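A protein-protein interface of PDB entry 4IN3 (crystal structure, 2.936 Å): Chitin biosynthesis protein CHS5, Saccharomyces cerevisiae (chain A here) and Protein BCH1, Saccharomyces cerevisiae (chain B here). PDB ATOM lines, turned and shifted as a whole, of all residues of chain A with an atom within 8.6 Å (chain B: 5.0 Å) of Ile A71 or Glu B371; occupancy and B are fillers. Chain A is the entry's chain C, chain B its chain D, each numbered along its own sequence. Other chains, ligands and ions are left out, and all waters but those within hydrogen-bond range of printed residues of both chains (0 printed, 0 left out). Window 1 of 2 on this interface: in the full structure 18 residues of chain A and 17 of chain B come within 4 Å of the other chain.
Of chain B, only Leu B368 and Glu B371 come within 4 Å of Ile A71. Of chain A, only His A67 (2.6 Å) and Ile A71 (3.9 Å) come within 4 Å of Glu B371. No residue of chain A comes within 4 Å of Lys B370. Printed residues of chain B within 4 Å of Phe A68: Glu B375 (3.9 Å). Printed residues of chain A within 4 Å of Leu B368: Ile A71 (3.9 Å) and Ile A75 (3.8 Å). Printed residues of chain A within 4 Å of Glu B375: Phe A68. Printed residues of chain B within 4 Å of Ile A75: Leu B368 and Val B372. The nearest residue of chain B that does not touch Ile A71 is Val B372 (4.2 Å).
A ring nitrogen (NE2) of His A67 is in hydrogen-bond range of the side-chain carboxylate (OE1) of Glu B371 (2.6 Å).
Among the printed residues, merely in contact across the chains: Ile A75 with Val B372, Ile A75 with Leu B368, Phe A68 with Glu B375, Ile A71 with Leu B368 and Ile A71 with Glu B371.
Hydrophobic or aromatic side chains of chain B that line the printed part of chain A: Leu B368 and Val B372. Printed residues of chain A that touch a printed residue of chain B: His A67, Phe A68, Ile A71 and Ile A75. Hydrophobic or aromatic side chains of chain A that line the printed part of chain B: His A67, Phe A68, Ile A71 and Ile A75. Among the printed residues, 6 pairs touch across the chains. Among the printed residues, no Asp or Glu carboxylate lies within 4 Å of a Lys or Arg side-chain nitrogen of the other chain.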
ATOM      1  N   GLN A  64       7.978  18.986   7.062  1.00  0.00           N
ATOM      2  CA  GLN A  64       6.804  18.267   7.544  1.00  0.00           C
ATOM      3  C   GLN A  64       6.017  17.641   6.392  1.00  0.00           C
ATOM      4  O   GLN A  64       5.257  16.692   6.594  1.00  0.00           O
ATOM      5  CB  GLN A  64       5.923  19.176   8.406  1.00  0.00           C
ATOM      6  CG  GLN A  64       6.713  19.935   9.466  1.00  0.00           C
ATOM      7  CD  GLN A  64       5.913  20.207  10.726  1.00  0.00           C
ATOM      8  OE1 GLN A  64       4.759  19.795  10.848  1.00  0.00           O
ATOM      9  NE2 GLN A  64       6.530  20.899  11.678  1.00  0.00           N
ATOM     10  N   ARG A  65       6.209  18.172   5.188  1.00  0.00           N
ATOM     11  CA  ARG A  65       5.632  17.580   3.987  1.00  0.00           C
ATOM     12  C   ARG A  65       6.251  16.214   3.732  1.00  0.00           C
ATOM     13  O   ARG A  65       5.548  15.203   3.642  1.00  0.00           O
ATOM     14  CB  ARG A  65       5.872  18.481   2.778  1.00  0.00           C
ATOM     15  CG  ARG A  65       5.494  17.854   1.449  1.00  0.00           C
ATOM     16  CD  ARG A  65       5.696  18.843   0.317  1.00  0.00           C
ATOM     17  NE  ARG A  65       5.083  20.132   0.624  1.00  0.00           N
ATOM     18  CZ  ARG A  65       5.738  21.288   0.642  1.00  0.00           C
ATOM     19  NH1 ARG A  65       7.032  21.326   0.352  1.00  0.00           N
ATOM     20  NH2 ARG A  65       5.095  22.408   0.940  1.00  0.00           N
ATOM     21  N   ASN A  66       7.577  16.198   3.611  1.00  0.00           N
ATOM     22  CA  ASN A  66       8.315  14.954   3.419  1.00  0.00           C
ATOM     23  C   ASN A  66       8.076  13.975   4.561  1.00  0.00           C
ATOM     24  O   ASN A  66       7.959  12.767   4.342  1.00  0.00           O
ATOM     25  CB  ASN A  66       9.811  15.235   3.258  1.00  0.00           C
ATOM     26  CG  ASN A  66      10.127  15.977   1.977  1.00  0.00           C
ATOM     27  OD1 ASN A  66       9.542  15.701   0.927  1.00  0.00           O
ATOM     28  ND2 ASN A  66      11.051  16.930   2.055  1.00  0.00           N
ATOM     29  N   HIS A  67       7.999  14.506   5.778  1.00  0.00           N
ATOM     30  CA  HIS A  67       7.726  13.695   6.955  1.00  0.00           C
ATOM     31  C   HIS A  67       6.379  12.996   6.829  1.00  0.00           C
ATOM     32  O   HIS A  67       6.283  11.779   6.994  1.00  0.00           O
ATOM     33  CB  HIS A  67       7.750  14.548   8.223  1.00  0.00           C
ATOM     34  CG  HIS A  67       7.318  13.811   9.451  1.00  0.00           C
ATOM     35  ND1 HIS A  67       8.133  12.913  10.106  1.00  0.00           N
ATOM     36  CD2 HIS A  67       6.151  13.830  10.136  1.00  0.00           C
ATOM     37  CE1 HIS A  67       7.487  12.415  11.147  1.00  0.00           C
ATOM     38  NE2 HIS A  67       6.283  12.954  11.186  1.00  0.00           N
ATOM     39  N   PHE A  68       5.344  13.775   6.530  1.00  0.00           N
ATOM     40  CA  PHE A  68       3.995  13.238   6.377  1.00  0.00           C
ATOM     41  C   PHE A  68       3.920  12.199   5.257  1.00  0.00           C
ATOM     42  O   PHE A  68       3.267  11.162   5.410  1.00  0.00           O
ATOM     43  CB  PHE A  68       2.996  14.373   6.133  1.00  0.00           C
ATOM     44  CG  PHE A  68       1.574  13.915   6.010  1.00  0.00           C
ATOM     45  CD1 PHE A  68       0.947  13.261   7.059  1.00  0.00           C
ATOM     46  CD2 PHE A  68       0.858  14.152   4.848  1.00  0.00           C
ATOM     47  CE1 PHE A  68      -0.366  12.842   6.947  1.00  0.00           C
ATOM     48  CE2 PHE A  68      -0.457  13.737   4.731  1.00  0.00           C
ATOM     49  CZ  PHE A  68      -1.069  13.081   5.782  1.00  0.00           C
ATOM     50  N   LYS A  69       4.587  12.480   4.138  1.00  0.00           N
ATOM     51  CA  LYS A  69       4.655  11.522   3.036  1.00  0.00           C
ATOM     52  C   LYS A  69       5.284  10.212   3.489  1.00  0.00           C
ATOM     53  O   LYS A  69       4.793   9.132   3.161  1.00  0.00           O
ATOM     54  CB  LYS A  69       5.455  12.084   1.862  1.00  0.00           C
ATOM     55  CG  LYS A  69       4.641  12.863   0.851  1.00  0.00           C
ATOM     56  CD  LYS A  69       5.513  13.240  -0.338  1.00  0.00           C
ATOM     57  CE  LYS A  69       4.975  14.463  -1.059  1.00  0.00           C
ATOM     58  NZ  LYS A  69       5.985  15.559  -1.100  1.00  0.00           N
ATOM     59  N   SER A  70       6.377  10.317   4.237  1.00  0.00           N
ATOM     60  CA  SER A  70       7.070   9.137   4.733  1.00  0.00           C
ATOM     61  C   SER A  70       6.168   8.335   5.669  1.00  0.00           C
ATOM     62  O   SER A  70       6.132   7.105   5.605  1.00  0.00           O
ATOM     63  CB  SER A  70       8.366   9.535   5.442  1.00  0.00           C
ATOM     64  OG  SER A  70       9.153   8.395   5.741  1.00  0.00           O
ATOM     65  N   ILE A  71       5.432   9.042   6.522  1.00  0.00           N
ATOM     66  CA  ILE A  71       4.474   8.415   7.429  1.00  0.00           C
ATOM     67  C   ILE A  71       3.404   7.637   6.668  1.00  0.00           C
ATOM     68  O   ILE A  71       3.184   6.454   6.929  1.00  0.00           O
ATOM     69  CB  ILE A  71       3.782   9.454   8.329  1.00  0.00           C
ATOM     70  CG1 ILE A  71       4.785  10.077   9.302  1.00  0.00           C
ATOM     71  CG2 ILE A  71       2.630   8.817   9.097  1.00  0.00           C
ATOM     72  CD1 ILE A  71       5.265   9.128  10.378  1.00  0.00           C
ATOM     73  N   GLN A  72       2.741   8.305   5.728  1.00  0.00           N
ATOM     74  CA  GLN A  72       1.692   7.666   4.935  1.00  0.00           C
ATOM     75  C   GLN A  72       2.215   6.473   4.137  1.00  0.00           C
ATOM     76  O   GLN A  72       1.542   5.441   4.034  1.00  0.00           O
ATOM     77  CB  GLN A  72       1.020   8.682   4.006  1.00  0.00           C
ATOM     78  CG  GLN A  72       0.074   9.639   4.720  1.00  0.00           C
ATOM     79  CD  GLN A  72      -1.185   8.952   5.220  1.00  0.00           C
ATOM     80  OE1 GLN A  72      -1.696   8.025   4.587  1.00  0.00           O
ATOM     81  NE2 GLN A  72      -1.691   9.406   6.363  1.00  0.00           N
ATOM     82  N   ALA A  73       3.416   6.616   3.580  1.00  0.00           N
ATOM     83  CA  ALA A  73       4.046   5.537   2.828  1.00  0.00           C
ATOM     84  C   ALA A  73       4.310   4.336   3.731  1.00  0.00           C
ATOM     85  O   ALA A  73       4.102   3.186   3.336  1.00  0.00           O
ATOM     86  CB  ALA A  73       5.334   6.018   2.191  1.00  0.00           C
ATOM     87  N   LYS A  74       4.768   4.616   4.949  1.00  0.00           N
ATOM     88  CA  LYS A  74       5.041   3.573   5.931  1.00  0.00           C
ATOM     89  C   LYS A  74       3.752   2.844   6.301  1.00  0.00           C
ATOM     90  O   LYS A  74       3.721   1.611   6.383  1.00  0.00           O
ATOM     91  CB  LYS A  74       5.678   4.174   7.185  1.00  0.00           C
ATOM     92  CG  LYS A  74       6.696   3.269   7.854  1.00  0.00           C
ATOM     93  CD  LYS A  74       8.046   3.378   7.163  1.00  0.00           C
ATOM     94  CE  LYS A  74       8.882   2.126   7.373  1.00  0.00           C
ATOM     95  NZ  LYS A  74      10.230   2.257   6.750  1.00  0.00           N
ATOM     96  N   ILE A  75       2.691   3.618   6.521  1.00  0.00           N
ATOM     97  CA  ILE A  75       1.376   3.067   6.831  1.00  0.00           C
ATOM     98  C   ILE A  75       0.890   2.150   5.709  1.00  0.00           C
ATOM     99  O   ILE A  75       0.369   1.064   5.968  1.00  0.00           O
ATOM    100  CB  ILE A  75       0.335   4.182   7.072  1.00  0.00           C
ATOM    101  CG1 ILE A  75       0.718   5.015   8.296  1.00  0.00           C
ATOM    102  CG2 ILE A  75      -1.051   3.591   7.261  1.00  0.00           C
ATOM    103  CD1 ILE A  75      -0.228   6.166   8.563  1.00  0.00           C
ATOM    104  N   LEU A  76       1.064   2.592   4.467  1.00  0.00           N
ATOM    105  CA  LEU A  76       0.691   1.781   3.311  1.00  0.00           C
ATOM    106  C   LEU A  76       1.500   0.490   3.253  1.00  0.00           C
ATOM    107  O   LEU A  76       0.966  -0.573   2.939  1.00  0.00           O
ATOM    108  CB  LEU A  76       0.886   2.569   2.015  1.00  0.00           C
ATOM    109  CG  LEU A  76       0.655   1.781   0.722  1.00  0.00           C
ATOM    110  CD1 LEU A  76      -0.810   1.405   0.577  1.00  0.00           C
ATOM    111  CD2 LEU A  76       1.142   2.555  -0.496  1.00  0.00           C
ATOM    112  N   GLU A  77       2.790   0.585   3.555  1.00  0.00           N
ATOM    113  CA  GLU A  77       3.667  -0.580   3.514  1.00  0.00           C
ATOM    114  C   GLU A  77       3.296  -1.631   4.562  1.00  0.00           C
ATOM    115  O   GLU A  77       3.173  -2.815   4.242  1.00  0.00           O
ATOM    116  CB  GLU A  77       5.128  -0.159   3.681  1.00  0.00           C
ATOM    117  CG  GLU A  77       6.104  -1.323   3.718  1.00  0.00           C
ATOM    118  CD  GLU A  77       7.545  -0.880   3.893  1.00  0.00           C
ATOM    119  OE1 GLU A  77       7.780   0.157   4.548  1.00  0.00           O
ATOM    120  OE2 GLU A  77       8.443  -1.574   3.370  1.00  0.00           O
ATOM    121  N   LYS A  78       3.115  -1.195   5.808  1.00  0.00           N
ATOM    122  CA  LYS A  78       2.797  -2.111   6.908  1.00  0.00           C
ATOM    123  C   LYS A  78       1.406  -2.740   6.807  1.00  0.00           C
ATOM    124  O   LYS A  78       1.179  -3.835   7.326  1.00  0.00           O
ATOM    125  CB  LYS A  78       2.920  -1.407   8.261  1.00  0.00           C
ATOM    126  CG  LYS A  78       4.327  -1.291   8.814  1.00  0.00           C
ATOM    127  CD  LYS A  78       4.256  -1.185  10.330  1.00  0.00           C
ATOM    128  CE  LYS A  78       5.370  -0.330  10.900  1.00  0.00           C
ATOM    129  NZ  LYS A  78       5.168  -0.113  12.362  1.00  0.00           N
ATOM    130  N   TYR A  79       0.479  -2.037   6.161  1.00  0.00           N
ATOM    131  CA  TYR A  79      -0.904  -2.495   6.033  1.00  0.00           C
ATOM    132  C   TYR A  79      -1.427  -2.226   4.622  1.00  0.00           C
ATOM    133  O   TYR A  79      -1.430  -1.081   4.171  1.00  0.00           O
ATOM    134  CB  TYR A  79      -1.801  -1.782   7.048  1.00  0.00           C
ATOM    135  CG  TYR A  79      -1.262  -1.752   8.459  1.00  0.00           C
ATOM    136  CD1 TYR A  79      -1.550  -2.774   9.354  1.00  0.00           C
ATOM    137  CD2 TYR A  79      -0.474  -0.699   8.898  1.00  0.00           C
ATOM    138  CE1 TYR A  79      -1.063  -2.748  10.646  1.00  0.00           C
ATOM    139  CE2 TYR A  79       0.018  -0.664  10.189  1.00  0.00           C
ATOM    140  CZ  TYR A  79      -0.280  -1.692  11.058  1.00  0.00           C
ATOM    141  OH  TYR A  79       0.206  -1.663  12.342  1.00  0.00           O
ATOM    142  N   LYS B 367       2.738   5.234  17.591  1.00  0.00           N
ATOM    143  CA  LYS B 367       3.549   6.298  17.010  1.00  0.00           C
ATOM    144  C   LYS B 367       2.941   6.842  15.714  1.00  0.00           C
ATOM    145  O   LYS B 367       2.749   8.052  15.574  1.00  0.00           O
ATOM    146  CB  LYS B 367       4.978   5.799  16.761  1.00  0.00           C
ATOM    147  CG  LYS B 367       5.673   5.233  17.997  1.00  0.00           C
ATOM    148  CD  LYS B 367       6.807   6.136  18.476  1.00  0.00           C
ATOM    149  CE  LYS B 367       6.282   7.403  19.138  1.00  0.00           C
ATOM    150  NZ  LYS B 367       7.388   8.340  19.498  1.00  0.00           N
ATOM    151  N   LEU B 368       2.638   5.948  14.773  1.00  0.00           N
ATOM    152  CA  LEU B 368       2.050   6.354  13.499  1.00  0.00           C
ATOM    153  C   LEU B 368       0.688   6.998  13.721  1.00  0.00           C
ATOM    154  O   LEU B 368       0.366   8.024  13.115  1.00  0.00           O
ATOM    155  CB  LEU B 368       1.923   5.165  12.543  1.00  0.00           C
ATOM    156  CG  LEU B 368       3.227   4.509  12.082  1.00  0.00           C
ATOM    157  CD1 LEU B 368       2.961   3.491  10.980  1.00  0.00           C
ATOM    158  CD2 LEU B 368       4.228   5.558  11.617  1.00  0.00           C
ATOM    159  N   ALA B 369      -0.098   6.394  14.606  1.00  0.00           N
ATOM    160  CA  ALA B 369      -1.401   6.935  14.970  1.00  0.00           C
ATOM    161  C   ALA B 369      -1.275   8.331  15.573  1.00  0.00           C
ATOM    162  O   ALA B 369      -2.143   9.178  15.369  1.00  0.00           O
ATOM    163  CB  ALA B 369      -2.118   6.002  15.935  1.00  0.00           C
ATOM    164  N   LYS B 370      -0.194   8.569  16.311  1.00  0.00           N
ATOM    165  CA  LYS B 370       0.051   9.888  16.883  1.00  0.00           C
ATOM    166  C   LYS B 370       0.352  10.883  15.776  1.00  0.00           C
ATOM    167  O   LYS B 370      -0.300  11.925  15.662  1.00  0.00           O
ATOM    168  CB  LYS B 370       1.228   9.850  17.858  1.00  0.00           C
ATOM    169  CG  LYS B 370       1.532  11.203  18.485  1.00  0.00           C
ATOM    170  CD  LYS B 370       2.956  11.268  19.022  1.00  0.00           C
ATOM    171  CE  LYS B 370       3.220  12.616  19.681  1.00  0.00           C
ATOM    172  NZ  LYS B 370       4.633  12.754  20.137  1.00  0.00           N
ATOM    173  N   GLU B 371       1.344  10.542  14.956  1.00  0.00           N
ATOM    174  CA  GLU B 371       1.776  11.397  13.852  1.00  0.00           C
ATOM    175  C   GLU B 371       0.649  11.698  12.863  1.00  0.00           C
ATOM    176  O   GLU B 371       0.694  12.706  12.157  1.00  0.00           O
ATOM    177  CB  GLU B 371       2.974  10.779  13.122  1.00  0.00           C
ATOM    178  CG  GLU B 371       4.216  10.647  13.990  1.00  0.00           C
ATOM    179  CD  GLU B 371       4.751  11.989  14.451  1.00  0.00           C
ATOM    180  OE1 GLU B 371       5.230  12.761  13.595  1.00  0.00           O
ATOM    181  OE2 GLU B 371       4.694  12.270  15.666  1.00  0.00           O
ATOM    182  N   VAL B 372      -0.358  10.827  12.816  1.00  0.00           N
ATOM    183  CA  VAL B 372      -1.528  11.063  11.974  1.00  0.00           C
ATOM    184  C   VAL B 372      -2.558  11.928  12.687  1.00  0.00           C
ATOM    185  O   VAL B 372      -3.017  12.932  12.141  1.00  0.00           O
ATOM    186  CB  VAL B 372      -2.187   9.744  11.511  1.00  0.00           C
ATOM    187  CG1 VAL B 372      -3.611   9.995  11.020  1.00  0.00           C
ATOM    188  CG2 VAL B 372      -1.356   9.092  10.424  1.00  0.00           C
ATOM    189  N   ALA B 373      -2.904  11.542  13.911  1.00  0.00           N
ATOM    190  CA  ALA B 373      -3.896  12.262  14.705  1.00  0.00           C
ATOM    191  C   ALA B 373      -3.514  13.720  14.955  1.00  0.00           C
ATOM    192  O   ALA B 373      -4.389  14.561  15.167  1.00  0.00           O
ATOM    193  CB  ALA B 373      -4.147  11.549  16.028  1.00  0.00           C
ATOM    194  N   MET B 374      -2.216  14.021  14.943  1.00  0.00           N
ATOM    195  CA  MET B 374      -1.781  15.410  15.068  1.00  0.00           C
ATOM    196  C   MET B 374      -2.191  16.207  13.832  1.00  0.00           C
ATOM    197  O   MET B 374      -2.669  17.337  13.940  1.00  0.00           O
ATOM    198  CB  MET B 374      -0.271  15.508  15.309  1.00  0.00           C
ATOM    199  CG  MET B 374       0.154  15.118  16.716  1.00  0.00           C
ATOM    200  SD  MET B 374       1.750  15.814  17.198  1.00  0.00           S
ATOM    201  CE  MET B 374       2.862  14.990  16.056  1.00  0.00           C
ATOM    202  N   GLU B 375      -2.002  15.608  12.660  1.00  0.00           N
ATOM    203  CA  GLU B 375      -2.441  16.207  11.404  1.00  0.00           C
ATOM    204  C   GLU B 375      -3.961  16.335  11.380  1.00  0.00           C
ATOM    205  O   GLU B 375      -4.508  17.319  10.875  1.00  0.00           O
ATOM    206  CB  GLU B 375      -1.964  15.366  10.215  1.00  0.00           C
ATOM    207  CG  GLU B 375      -0.472  15.468   9.927  1.00  0.00           C
ATOM    208  CD  GLU B 375      -0.133  16.631   9.014  1.00  0.00           C
ATOM    209  OE1 GLU B 375      -0.696  16.697   7.900  1.00  0.00           O
ATOM    210  OE2 GLU B 375       0.691  17.484   9.410  1.00  0.00           O
